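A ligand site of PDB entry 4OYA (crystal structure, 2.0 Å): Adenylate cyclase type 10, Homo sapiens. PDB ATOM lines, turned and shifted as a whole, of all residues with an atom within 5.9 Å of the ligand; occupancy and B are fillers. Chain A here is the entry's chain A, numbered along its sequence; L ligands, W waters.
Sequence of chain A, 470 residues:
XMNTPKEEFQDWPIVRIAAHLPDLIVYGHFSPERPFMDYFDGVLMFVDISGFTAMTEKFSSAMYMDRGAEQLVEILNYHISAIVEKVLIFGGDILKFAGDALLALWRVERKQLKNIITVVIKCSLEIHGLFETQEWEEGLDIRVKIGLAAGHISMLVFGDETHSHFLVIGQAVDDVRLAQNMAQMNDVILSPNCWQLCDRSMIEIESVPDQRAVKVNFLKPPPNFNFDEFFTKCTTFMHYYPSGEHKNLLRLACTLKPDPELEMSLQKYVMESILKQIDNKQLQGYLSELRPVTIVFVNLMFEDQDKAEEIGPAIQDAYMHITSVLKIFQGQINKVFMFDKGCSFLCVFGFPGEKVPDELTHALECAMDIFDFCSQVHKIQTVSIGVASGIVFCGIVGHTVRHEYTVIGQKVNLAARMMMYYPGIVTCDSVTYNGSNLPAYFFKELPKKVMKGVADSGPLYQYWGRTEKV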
ATOM      1  N   PHE A  46     -14.207 -17.142  15.111  1.00  0.00           N
ATOM      2  CA  PHE A  46     -13.572 -18.448  14.931  1.00  0.00           C
ATOM      3  C   PHE A  46     -14.595 -19.393  14.375  1.00  0.00           C
ATOM      4  O   PHE A  46     -15.578 -19.701  15.049  1.00  0.00           O
ATOM      5  CB  PHE A  46     -13.011 -18.956  16.271  1.00  0.00           C
ATOM      6  CG  PHE A  46     -11.880 -19.954  16.141  1.00  0.00           C
ATOM      7  CD1 PHE A  46     -10.841 -19.733  15.255  1.00  0.00           C
ATOM      8  CD2 PHE A  46     -11.849 -21.087  16.936  1.00  0.00           C
ATOM      9  CE1 PHE A  46      -9.796 -20.645  15.141  1.00  0.00           C
ATOM     10  CE2 PHE A  46     -10.804 -21.999  16.822  1.00  0.00           C
ATOM     11  CZ  PHE A  46      -9.788 -21.773  15.943  1.00  0.00           C
ATOM     12  N   LEU A  95      -7.779 -13.898   8.778  1.00  0.00           N
ATOM     13  CA  LEU A  95      -6.368 -13.914   9.229  1.00  0.00           C
ATOM     14  C   LEU A  95      -5.642 -15.167   8.782  1.00  0.00           C
ATOM     15  O   LEU A  95      -4.533 -15.066   8.270  1.00  0.00           O
ATOM     16  CB  LEU A  95      -6.254 -13.812  10.740  1.00  0.00           C
ATOM     17  CG  LEU A  95      -6.772 -12.536  11.379  1.00  0.00           C
ATOM     18  CD1 LEU A  95      -6.420 -12.542  12.862  1.00  0.00           C
ATOM     19  CD2 LEU A  95      -6.190 -11.263  10.636  1.00  0.00           C
ATOM     20  N   LYS A  96      -6.279 -16.333   8.949  1.00  0.00           N
ATOM     21  CA  LYS A  96      -5.605 -17.627   8.734  1.00  0.00           C
ATOM     22  C   LYS A  96      -6.599 -18.767   8.572  1.00  0.00           C
ATOM     23  O   LYS A  96      -7.672 -18.714   9.171  1.00  0.00           O
ATOM     24  CB  LYS A  96      -4.738 -17.915   9.991  1.00  0.00           C
ATOM     25  CG  LYS A  96      -3.512 -18.739   9.716  1.00  0.00           C
ATOM     26  CD  LYS A  96      -2.525 -18.700  10.883  1.00  0.00           C
ATOM     27  CE  LYS A  96      -1.678 -17.448  10.923  1.00  0.00           C
ATOM     28  NZ  LYS A  96      -0.377 -17.694  11.604  1.00  0.00           N
ATOM     29  N   PHE A  97      -6.219 -19.771   7.775  1.00  0.00           N
ATOM     30  CA  PHE A  97      -6.934 -21.019   7.611  1.00  0.00           C
ATOM     31  C   PHE A  97      -6.139 -22.144   8.256  1.00  0.00           C
ATOM     32  O   PHE A  97      -4.914 -22.167   8.205  1.00  0.00           O
ATOM     33  CB  PHE A  97      -7.187 -21.383   6.141  1.00  0.00           C
ATOM     34  CG  PHE A  97      -7.958 -20.412   5.285  1.00  0.00           C
ATOM     35  CD1 PHE A  97      -7.328 -19.298   4.729  1.00  0.00           C
ATOM     36  CD2 PHE A  97      -9.309 -20.617   5.007  1.00  0.00           C
ATOM     37  CE1 PHE A  97      -8.048 -18.404   3.904  1.00  0.00           C
ATOM     38  CE2 PHE A  97     -10.024 -19.731   4.202  1.00  0.00           C
ATOM     39  CZ  PHE A  97      -9.394 -18.632   3.655  1.00  0.00           C
ATOM     40  N   ALA A  98      -6.856 -23.063   8.887  1.00  0.00           N
ATOM     41  CA  ALA A  98      -6.306 -24.361   9.313  1.00  0.00           C
ATOM     42  C   ALA A  98      -7.245 -25.421   8.770  1.00  0.00           C
ATOM     43  O   ALA A  98      -8.370 -25.094   8.331  1.00  0.00           O
ATOM     44  CB  ALA A  98      -6.260 -24.427  10.822  1.00  0.00           C
ATOM     45  N   ASP A 100      -9.058 -27.372  10.438  1.00  0.00           N
ATOM     46  CA  ASP A 100     -10.232 -27.489  11.324  1.00  0.00           C
ATOM     47  C   ASP A 100     -10.994 -26.143  11.531  1.00  0.00           C
ATOM     48  O   ASP A 100     -12.129 -26.185  11.993  1.00  0.00           O
ATOM     49  CB  ASP A 100      -9.746 -27.989  12.685  1.00  0.00           C
ATOM     50  CG  ASP A 100      -8.821 -26.982  13.354  1.00  0.00           C
ATOM     51  OD1 ASP A 100      -7.751 -26.673  12.773  1.00  0.00           O
ATOM     52  OD2 ASP A 100      -9.230 -26.401  14.398  1.00  0.00           O
ATOM     53  N   ALA A 101     -10.379 -24.983  11.219  1.00  0.00           N
ATOM     54  CA  ALA A 101     -10.967 -23.679  11.476  1.00  0.00           C
ATOM     55  C   ALA A 101     -10.453 -22.541  10.562  1.00  0.00           C
ATOM     56  O   ALA A 101      -9.377 -22.636   9.959  1.00  0.00           O
ATOM     57  CB  ALA A 101     -10.751 -23.281  12.933  1.00  0.00           C
ATOM     58  N   LEU A 102     -11.251 -21.469  10.469  1.00  0.00           N
ATOM     59  CA  LEU A 102     -10.717 -20.199  10.023  1.00  0.00           C
ATOM     60  C   LEU A 102     -10.948 -19.129  11.058  1.00  0.00           C
ATOM     61  O   LEU A 102     -11.928 -19.188  11.813  1.00  0.00           O
ATOM     62  CB  LEU A 102     -11.185 -19.787   8.627  1.00  0.00           C
ATOM     63  CG  LEU A 102     -12.642 -19.505   8.384  1.00  0.00           C
ATOM     64  CD1 LEU A 102     -12.956 -18.036   8.700  1.00  0.00           C
ATOM     65  CD2 LEU A 102     -12.952 -19.738   6.907  1.00  0.00           C
ATOM     66  N   LEU A 103     -10.055 -18.159  11.103  1.00  0.00           N
ATOM     67  CA  LEU A 103     -10.112 -17.093  12.070  1.00  0.00           C
ATOM     68  C   LEU A 103     -10.226 -15.792  11.327  1.00  0.00           C
ATOM     69  O   LEU A 103      -9.448 -15.552  10.408  1.00  0.00           O
ATOM     70  CB  LEU A 103      -8.820 -17.109  12.919  1.00  0.00           C
ATOM     71  CG  LEU A 103      -8.690 -16.004  14.016  1.00  0.00           C
ATOM     72  CD1 LEU A 103      -9.771 -16.195  15.141  1.00  0.00           C
ATOM     73  CD2 LEU A 103      -7.309 -16.041  14.643  1.00  0.00           C
ATOM     74  N   PHE A 166       3.242 -14.502  11.318  1.00  0.00           N
ATOM     75  CA  PHE A 166       2.552 -13.668  12.314  1.00  0.00           C
ATOM     76  C   PHE A 166       1.581 -14.513  13.139  1.00  0.00           C
ATOM     77  O   PHE A 166       1.183 -15.615  12.736  1.00  0.00           O
ATOM     78  CB  PHE A 166       1.807 -12.488  11.639  1.00  0.00           C
ATOM     79  CG  PHE A 166       0.453 -12.900  11.061  1.00  0.00           C
ATOM     80  CD1 PHE A 166      -0.718 -12.766  11.816  1.00  0.00           C
ATOM     81  CD2 PHE A 166       0.370 -13.435   9.784  1.00  0.00           C
ATOM     82  CE1 PHE A 166      -1.957 -13.166  11.285  1.00  0.00           C
ATOM     83  CE2 PHE A 166      -0.876 -13.829   9.252  1.00  0.00           C
ATOM     84  CZ  PHE A 166      -2.027 -13.686  10.010  1.00  0.00           C
ATOM     85  N   LEU A 167       1.187 -13.952  14.285  1.00  0.00           N
ATOM     86  CA  LEU A 167       0.201 -14.491  15.193  1.00  0.00           C
ATOM     87  C   LEU A 167      -0.578 -13.331  15.808  1.00  0.00           C
ATOM     88  O   LEU A 167      -0.009 -12.261  16.019  1.00  0.00           O
ATOM     89  CB  LEU A 167       0.908 -15.224  16.353  1.00  0.00           C
ATOM     90  CG  LEU A 167       1.451 -16.610  16.093  1.00  0.00           C
ATOM     91  CD1 LEU A 167       2.300 -17.088  17.303  1.00  0.00           C
ATOM     92  CD2 LEU A 167       0.330 -17.601  15.804  1.00  0.00           C
ATOM     93  N   VAL A 168      -1.869 -13.549  16.083  1.00  0.00           N
ATOM     94  CA  VAL A 168      -2.611 -12.702  17.033  1.00  0.00           C
ATOM     95  C   VAL A 168      -2.659 -13.478  18.341  1.00  0.00           C
ATOM     96  O   VAL A 168      -2.833 -14.706  18.342  1.00  0.00           O
ATOM     97  CB  VAL A 168      -4.025 -12.251  16.555  1.00  0.00           C
ATOM     98  CG1 VAL A 168      -3.925 -11.235  15.434  1.00  0.00           C
ATOM     99  CG2 VAL A 168      -4.906 -13.431  16.162  1.00  0.00           C
ATOM    100  N   ILE A 169      -2.517 -12.751  19.470  1.00  0.00           N
ATOM    101  CA  ILE A 169      -2.419 -13.361  20.791  1.00  0.00           C
ATOM    102  C   ILE A 169      -3.160 -12.447  21.807  1.00  0.00           C
ATOM    103  O   ILE A 169      -3.527 -11.313  21.472  1.00  0.00           O
ATOM    104  CB  ILE A 169      -0.921 -13.675  21.220  1.00  0.00           C
ATOM    105  CG1 ILE A 169      -0.154 -12.415  21.573  1.00  0.00           C
ATOM    106  CG2 ILE A 169      -0.123 -14.496  20.159  1.00  0.00           C
ATOM    107  CD1 ILE A 169       0.691 -12.566  22.768  1.00  0.00           C
ATOM    108  N   VAL A 173      -8.152 -13.504  21.865  1.00  0.00           N
ATOM    109  CA  VAL A 173      -7.705 -14.700  21.132  1.00  0.00           C
ATOM    110  C   VAL A 173      -7.957 -15.970  21.970  1.00  0.00           C
ATOM    111  O   VAL A 173      -8.548 -16.922  21.451  1.00  0.00           O
ATOM    112  CB  VAL A 173      -6.222 -14.549  20.685  1.00  0.00           C
ATOM    113  CG1 VAL A 173      -5.684 -15.847  20.067  1.00  0.00           C
ATOM    114  CG2 VAL A 173      -6.075 -13.411  19.691  1.00  0.00           C
ATOM    115  N   ARG A 177     -11.262 -19.048  21.234  1.00  0.00           N
ATOM    116  CA  ARG A 177     -11.137 -20.496  21.237  1.00  0.00           C
ATOM    117  C   ARG A 177     -11.983 -21.150  22.317  1.00  0.00           C
ATOM    118  O   ARG A 177     -12.618 -22.163  22.031  1.00  0.00           O
ATOM    119  CB  ARG A 177      -9.679 -20.957  21.295  1.00  0.00           C
ATOM    120  CG  ARG A 177      -9.375 -21.907  20.147  1.00  0.00           C
ATOM    121  CD  ARG A 177      -9.494 -23.377  20.521  1.00  0.00           C
ATOM    122  NE  ARG A 177      -9.685 -24.225  19.336  1.00  0.00           N
ATOM    123  CZ  ARG A 177      -8.706 -24.729  18.587  1.00  0.00           C
ATOM    124  NH1 ARG A 177      -7.433 -24.474  18.889  1.00  0.00           N
ATOM    125  NH2 ARG A 177      -8.978 -25.493  17.539  1.00  0.00           N
ATOM    126  N   PHE A 297       4.631 -31.658  15.240  1.00  0.00           N
ATOM    127  CA  PHE A 297       3.834 -30.598  15.824  1.00  0.00           C
ATOM    128  C   PHE A 297       4.489 -30.167  17.150  1.00  0.00           C
ATOM    129  O   PHE A 297       4.485 -30.917  18.132  1.00  0.00           O
ATOM    130  CB  PHE A 297       2.357 -31.035  15.997  1.00  0.00           C
ATOM    131  CG  PHE A 297       1.306 -30.020  15.541  1.00  0.00           C
ATOM    132  CD1 PHE A 297       1.438 -28.666  15.838  1.00  0.00           C
ATOM    133  CD2 PHE A 297       0.196 -30.439  14.803  1.00  0.00           C
ATOM    134  CE1 PHE A 297       0.468 -27.725  15.398  1.00  0.00           C
ATOM    135  CE2 PHE A 297      -0.776 -29.513  14.392  1.00  0.00           C
ATOM    136  CZ  PHE A 297      -0.630 -28.159  14.691  1.00  0.00           C
ATOM    137  N   VAL A 336       1.668 -21.584  12.006  1.00  0.00           N
ATOM    138  CA  VAL A 336       1.895 -21.238  13.409  1.00  0.00           C
ATOM    139  C   VAL A 336       0.546 -20.772  14.004  1.00  0.00           C
ATOM    140  O   VAL A 336      -0.155 -19.977  13.397  1.00  0.00           O
ATOM    141  CB  VAL A 336       3.036 -20.200  13.644  1.00  0.00           C
ATOM    142  CG1 VAL A 336       3.431 -20.159  15.107  1.00  0.00           C
ATOM    143  CG2 VAL A 336       4.260 -20.493  12.783  1.00  0.00           C
ATOM    144  N   PHE A 337       0.194 -21.283  15.172  1.00  0.00           N
ATOM    145  CA  PHE A 337      -1.089 -21.024  15.851  1.00  0.00           C
ATOM    146  C   PHE A 337      -0.787 -20.790  17.286  1.00  0.00           C
ATOM    147  O   PHE A 337       0.206 -21.322  17.791  1.00  0.00           O
ATOM    148  CB  PHE A 337      -2.010 -22.268  15.831  1.00  0.00           C
ATOM    149  CG  PHE A 337      -2.338 -22.903  14.503  1.00  0.00           C
ATOM    150  CD1 PHE A 337      -2.170 -24.271  14.316  1.00  0.00           C
ATOM    151  CD2 PHE A 337      -2.848 -22.135  13.453  1.00  0.00           C
ATOM    152  CE1 PHE A 337      -2.493 -24.863  13.093  1.00  0.00           C
ATOM    153  CE2 PHE A 337      -3.171 -22.727  12.230  1.00  0.00           C
ATOM    154  CZ  PHE A 337      -2.999 -24.088  12.064  1.00  0.00           C
ATOM    155  N   MET A 338      -1.671 -20.032  17.956  1.00  0.00           N
ATOM    156  CA  MET A 338      -1.551 -19.747  19.391  1.00  0.00           C
ATOM    157  C   MET A 338      -2.895 -19.406  20.058  1.00  0.00           C
ATOM    158  O   MET A 338      -3.536 -18.451  19.663  1.00  0.00           O
ATOM    159  CB  MET A 338      -0.522 -18.623  19.617  1.00  0.00           C
ATOM    160  CG  MET A 338      -0.439 -18.183  21.040  1.00  0.00           C
ATOM    161  SD  MET A 338       1.222 -17.682  21.372  1.00  0.00           S
ATOM    162  CE  MET A 338       1.082 -17.486  23.120  1.00  0.00           C
ATOM    163  N   PHE A 339      -3.319 -20.175  21.084  1.00  0.00           N
ATOM    164  CA  PHE A 339      -4.559 -19.895  21.810  1.00  0.00           C
ATOM    165  C   PHE A 339      -4.455 -20.062  23.299  1.00  0.00           C
ATOM    166  O   PHE A 339      -4.448 -19.064  23.986  1.00  0.00           O
ATOM    167  CB  PHE A 339      -5.753 -20.712  21.293  1.00  0.00           C
ATOM    168  CG  PHE A 339      -6.275 -20.342  19.937  1.00  0.00           C
ATOM    169  CD1 PHE A 339      -6.172 -21.227  18.869  1.00  0.00           C
ATOM    170  CD2 PHE A 339      -6.879 -19.106  19.721  1.00  0.00           C
ATOM    171  CE1 PHE A 339      -6.670 -20.884  17.615  1.00  0.00           C
ATOM    172  CE2 PHE A 339      -7.361 -18.760  18.449  1.00  0.00           C
ATOM    173  CZ  PHE A 339      -7.248 -19.647  17.412  1.00  0.00           C
ATOM    174  N   SER A 344       2.128 -23.018  18.815  1.00  0.00           N
ATOM    175  CA  SER A 344       2.259 -24.326  18.143  1.00  0.00           C
ATOM    176  C   SER A 344       2.756 -24.156  16.704  1.00  0.00           C
ATOM    177  O   SER A 344       2.165 -23.398  15.936  1.00  0.00           O
ATOM    178  CB  SER A 344       0.915 -25.067  18.107  1.00  0.00           C
ATOM    179  OG  SER A 344       0.547 -25.496  19.410  1.00  0.00           O
ATOM    180  N   ALA A 416      -1.152 -33.170  16.826  1.00  0.00           N
ATOM    181  CA  ALA A 416      -1.654 -32.031  17.618  1.00  0.00           C
ATOM    182  C   ALA A 416      -2.172 -32.518  18.988  1.00  0.00           C
ATOM    183  O   ALA A 416      -1.888 -31.880  20.007  1.00  0.00           O
ATOM    184  CB  ALA A 416      -2.766 -31.319  16.858  1.00  0.00           C
ATOM    185  N   MET A 419       0.898 -33.829  21.369  1.00  0.00           N
ATOM    186  CA  MET A 419       1.679 -32.774  22.023  1.00  0.00           C
ATOM    187  C   MET A 419       0.909 -32.152  23.224  1.00  0.00           C
ATOM    188  O   MET A 419       1.535 -31.704  24.183  1.00  0.00           O
ATOM    189  CB  MET A 419       2.205 -31.735  21.011  1.00  0.00           C
ATOM    190  CG  MET A 419       1.206 -30.668  20.679  1.00  0.00           C
ATOM    191  SD  MET A 419       1.543 -29.633  19.227  1.00  0.00           S
ATOM    192  CE  MET A 419      -0.041 -28.846  19.158  1.00  0.00           C
HETATM  193  C1  LIG L   1      -3.390 -17.040  15.766  1.00  0.00           C
HETATM  194  C2  LIG L   1      -3.946 -17.937  14.811  1.00  0.00           C
HETATM  195  C3  LIG L   1      -4.578 -19.254  15.109  1.00  0.00           C
HETATM  196  C4  LIG L   1      -5.981 -19.364  13.000  1.00  0.00           C
HETATM  197  C5  LIG L   1      -6.829 -20.069  12.153  1.00  0.00           C
HETATM  198  C6  LIG L   1      -7.190 -21.366  12.447  1.00  0.00           C
HETATM  199  C7  LIG L   1      -6.696 -21.964  13.589  1.00  0.00           C
HETATM  200  C8  LIG L   1      -7.341 -23.685  15.189  1.00  0.00           C
HETATM  201  C9  LIG L   1      -6.202 -24.473  15.734  1.00  0.00           C
HETATM  202  C10 LIG L   1      -3.416 -25.249  17.806  1.00  0.00           C
HETATM  203  C11 LIG L   1      -3.007 -27.464  16.978  1.00  0.00           C
HETATM  204  C12 LIG L   1      -4.072 -27.344  16.096  1.00  0.00           C
HETATM  205  C13 LIG L   1      -4.814 -26.159  16.070  1.00  0.00           C
HETATM  206  C14 LIG L   1      -5.879 -21.262  14.452  1.00  0.00           C
HETATM  207  N1  LIG L   1      -3.374 -17.196  17.112  1.00  0.00           N
HETATM  208  N2  LIG L   1      -2.912 -15.997  15.153  1.00  0.00           N
HETATM  209  O1  LIG L   1      -3.143 -16.219  13.820  1.00  0.00           O
HETATM  210  N3  LIG L   1      -3.776 -17.437  13.619  1.00  0.00           N
HETATM  211  O2  LIG L   1      -4.317 -19.772  16.186  1.00  0.00           O
HETATM  212  C15 LIG L   1      -5.498 -19.957  14.161  1.00  0.00           C
HETATM  213  O3  LIG L   1      -7.108 -23.276  13.845  1.00  0.00           O
HETATM  214  N4  LIG L   1      -5.380 -24.090  16.704  1.00  0.00           N
HETATM  215  C16 LIG L   1      -4.494 -25.129  16.913  1.00  0.00           C
HETATM  216  C17 LIG L   1      -2.674 -26.419  17.823  1.00  0.00           C
HETATM  217  N5  LIG L   1      -5.885 -25.731  15.353  1.00  0.00           N
HETATM  218  O   HOH W   1      -1.421 -23.241  19.699  1.00  0.00           O
HETATM  219  O   HOH W   2      -4.124 -24.111  20.959  1.00  0.00           O
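Water W1 bridges the side-chain hydroxyl of Ser 344 and the backbone carbonyl oxygen of Phe 337.
Merely in contact with the ligand: Phe 339, Phe 46, Lys 96, Phe 337, Ala 98, Phe 297, Leu 167, Ala 101, Leu 103, Ser 344, Met 419, Ala 416 and Val 173.
17 residues have an atom within 4 Å of the ligand: Phe 46, Lys 96, Ala 98, Asp 100, Ala 101, Leu 103, Leu 167, Val 168, Val 173, Arg 177, Phe 297, Phe 337, Met 338, Phe 339, Ser 344, Ala 416 and Met 419.
Along chain A the residues within 4 Å of the ligand span positions 46 to 419.
NH2 of Arg 177 is in salt-bridge range of OD2 of Asp 100 (3.3 Å).
The backbone carbonyl oxygen (O) of Lys 96 is in hydrogen-bond range of the backbone NH (N) of Leu 103 (3.1 Å).
The side-chain amino group of Lys 96 is in hydrogen-bond range of the backbone carbonyl oxygen of Phe 166 (2.8 Å).
The backbone carbonyl oxygen (O) of Val 336 sits at hydrogen-bond distance from the side-chain amino group (NZ) of Lys 96 (2.9 Å).
The backbone carbonyl oxygen (O) of Phe 337 lies within hydrogen-bond range of the backbone NH (N) of Ser 344, 2.8 Å away.
O of Leu 103 lies within hydrogen-bond range of N of Leu 95, at 2.9 Å.
N of Val 168 is in hydrogen-bond range of N2 of the ligand (2.8 Å).
The backbone carbonyl oxygen of Val 168 lies within hydrogen-bond range of a nitrogen (N1) of the ligand (2.8 Å).
The backbone NH (N) of Met 338 is in hydrogen-bond range of an oxygen (O2) of the ligand (3.2 Å).
A nitrogen (N1) of the ligand is in hydrogen-bond range of the backbone carbonyl oxygen of Met 338 (2.8 Å).
The guanidinium group (NH1) of Arg 177 sits at hydrogen-bond distance from a nitrogen (N4) of the ligand, at 3.0 Å.
The side-chain carboxylate (OD1) of Asp 100 lies within hydrogen-bond range of a nitrogen (N5) of the ligand (3.3 Å).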
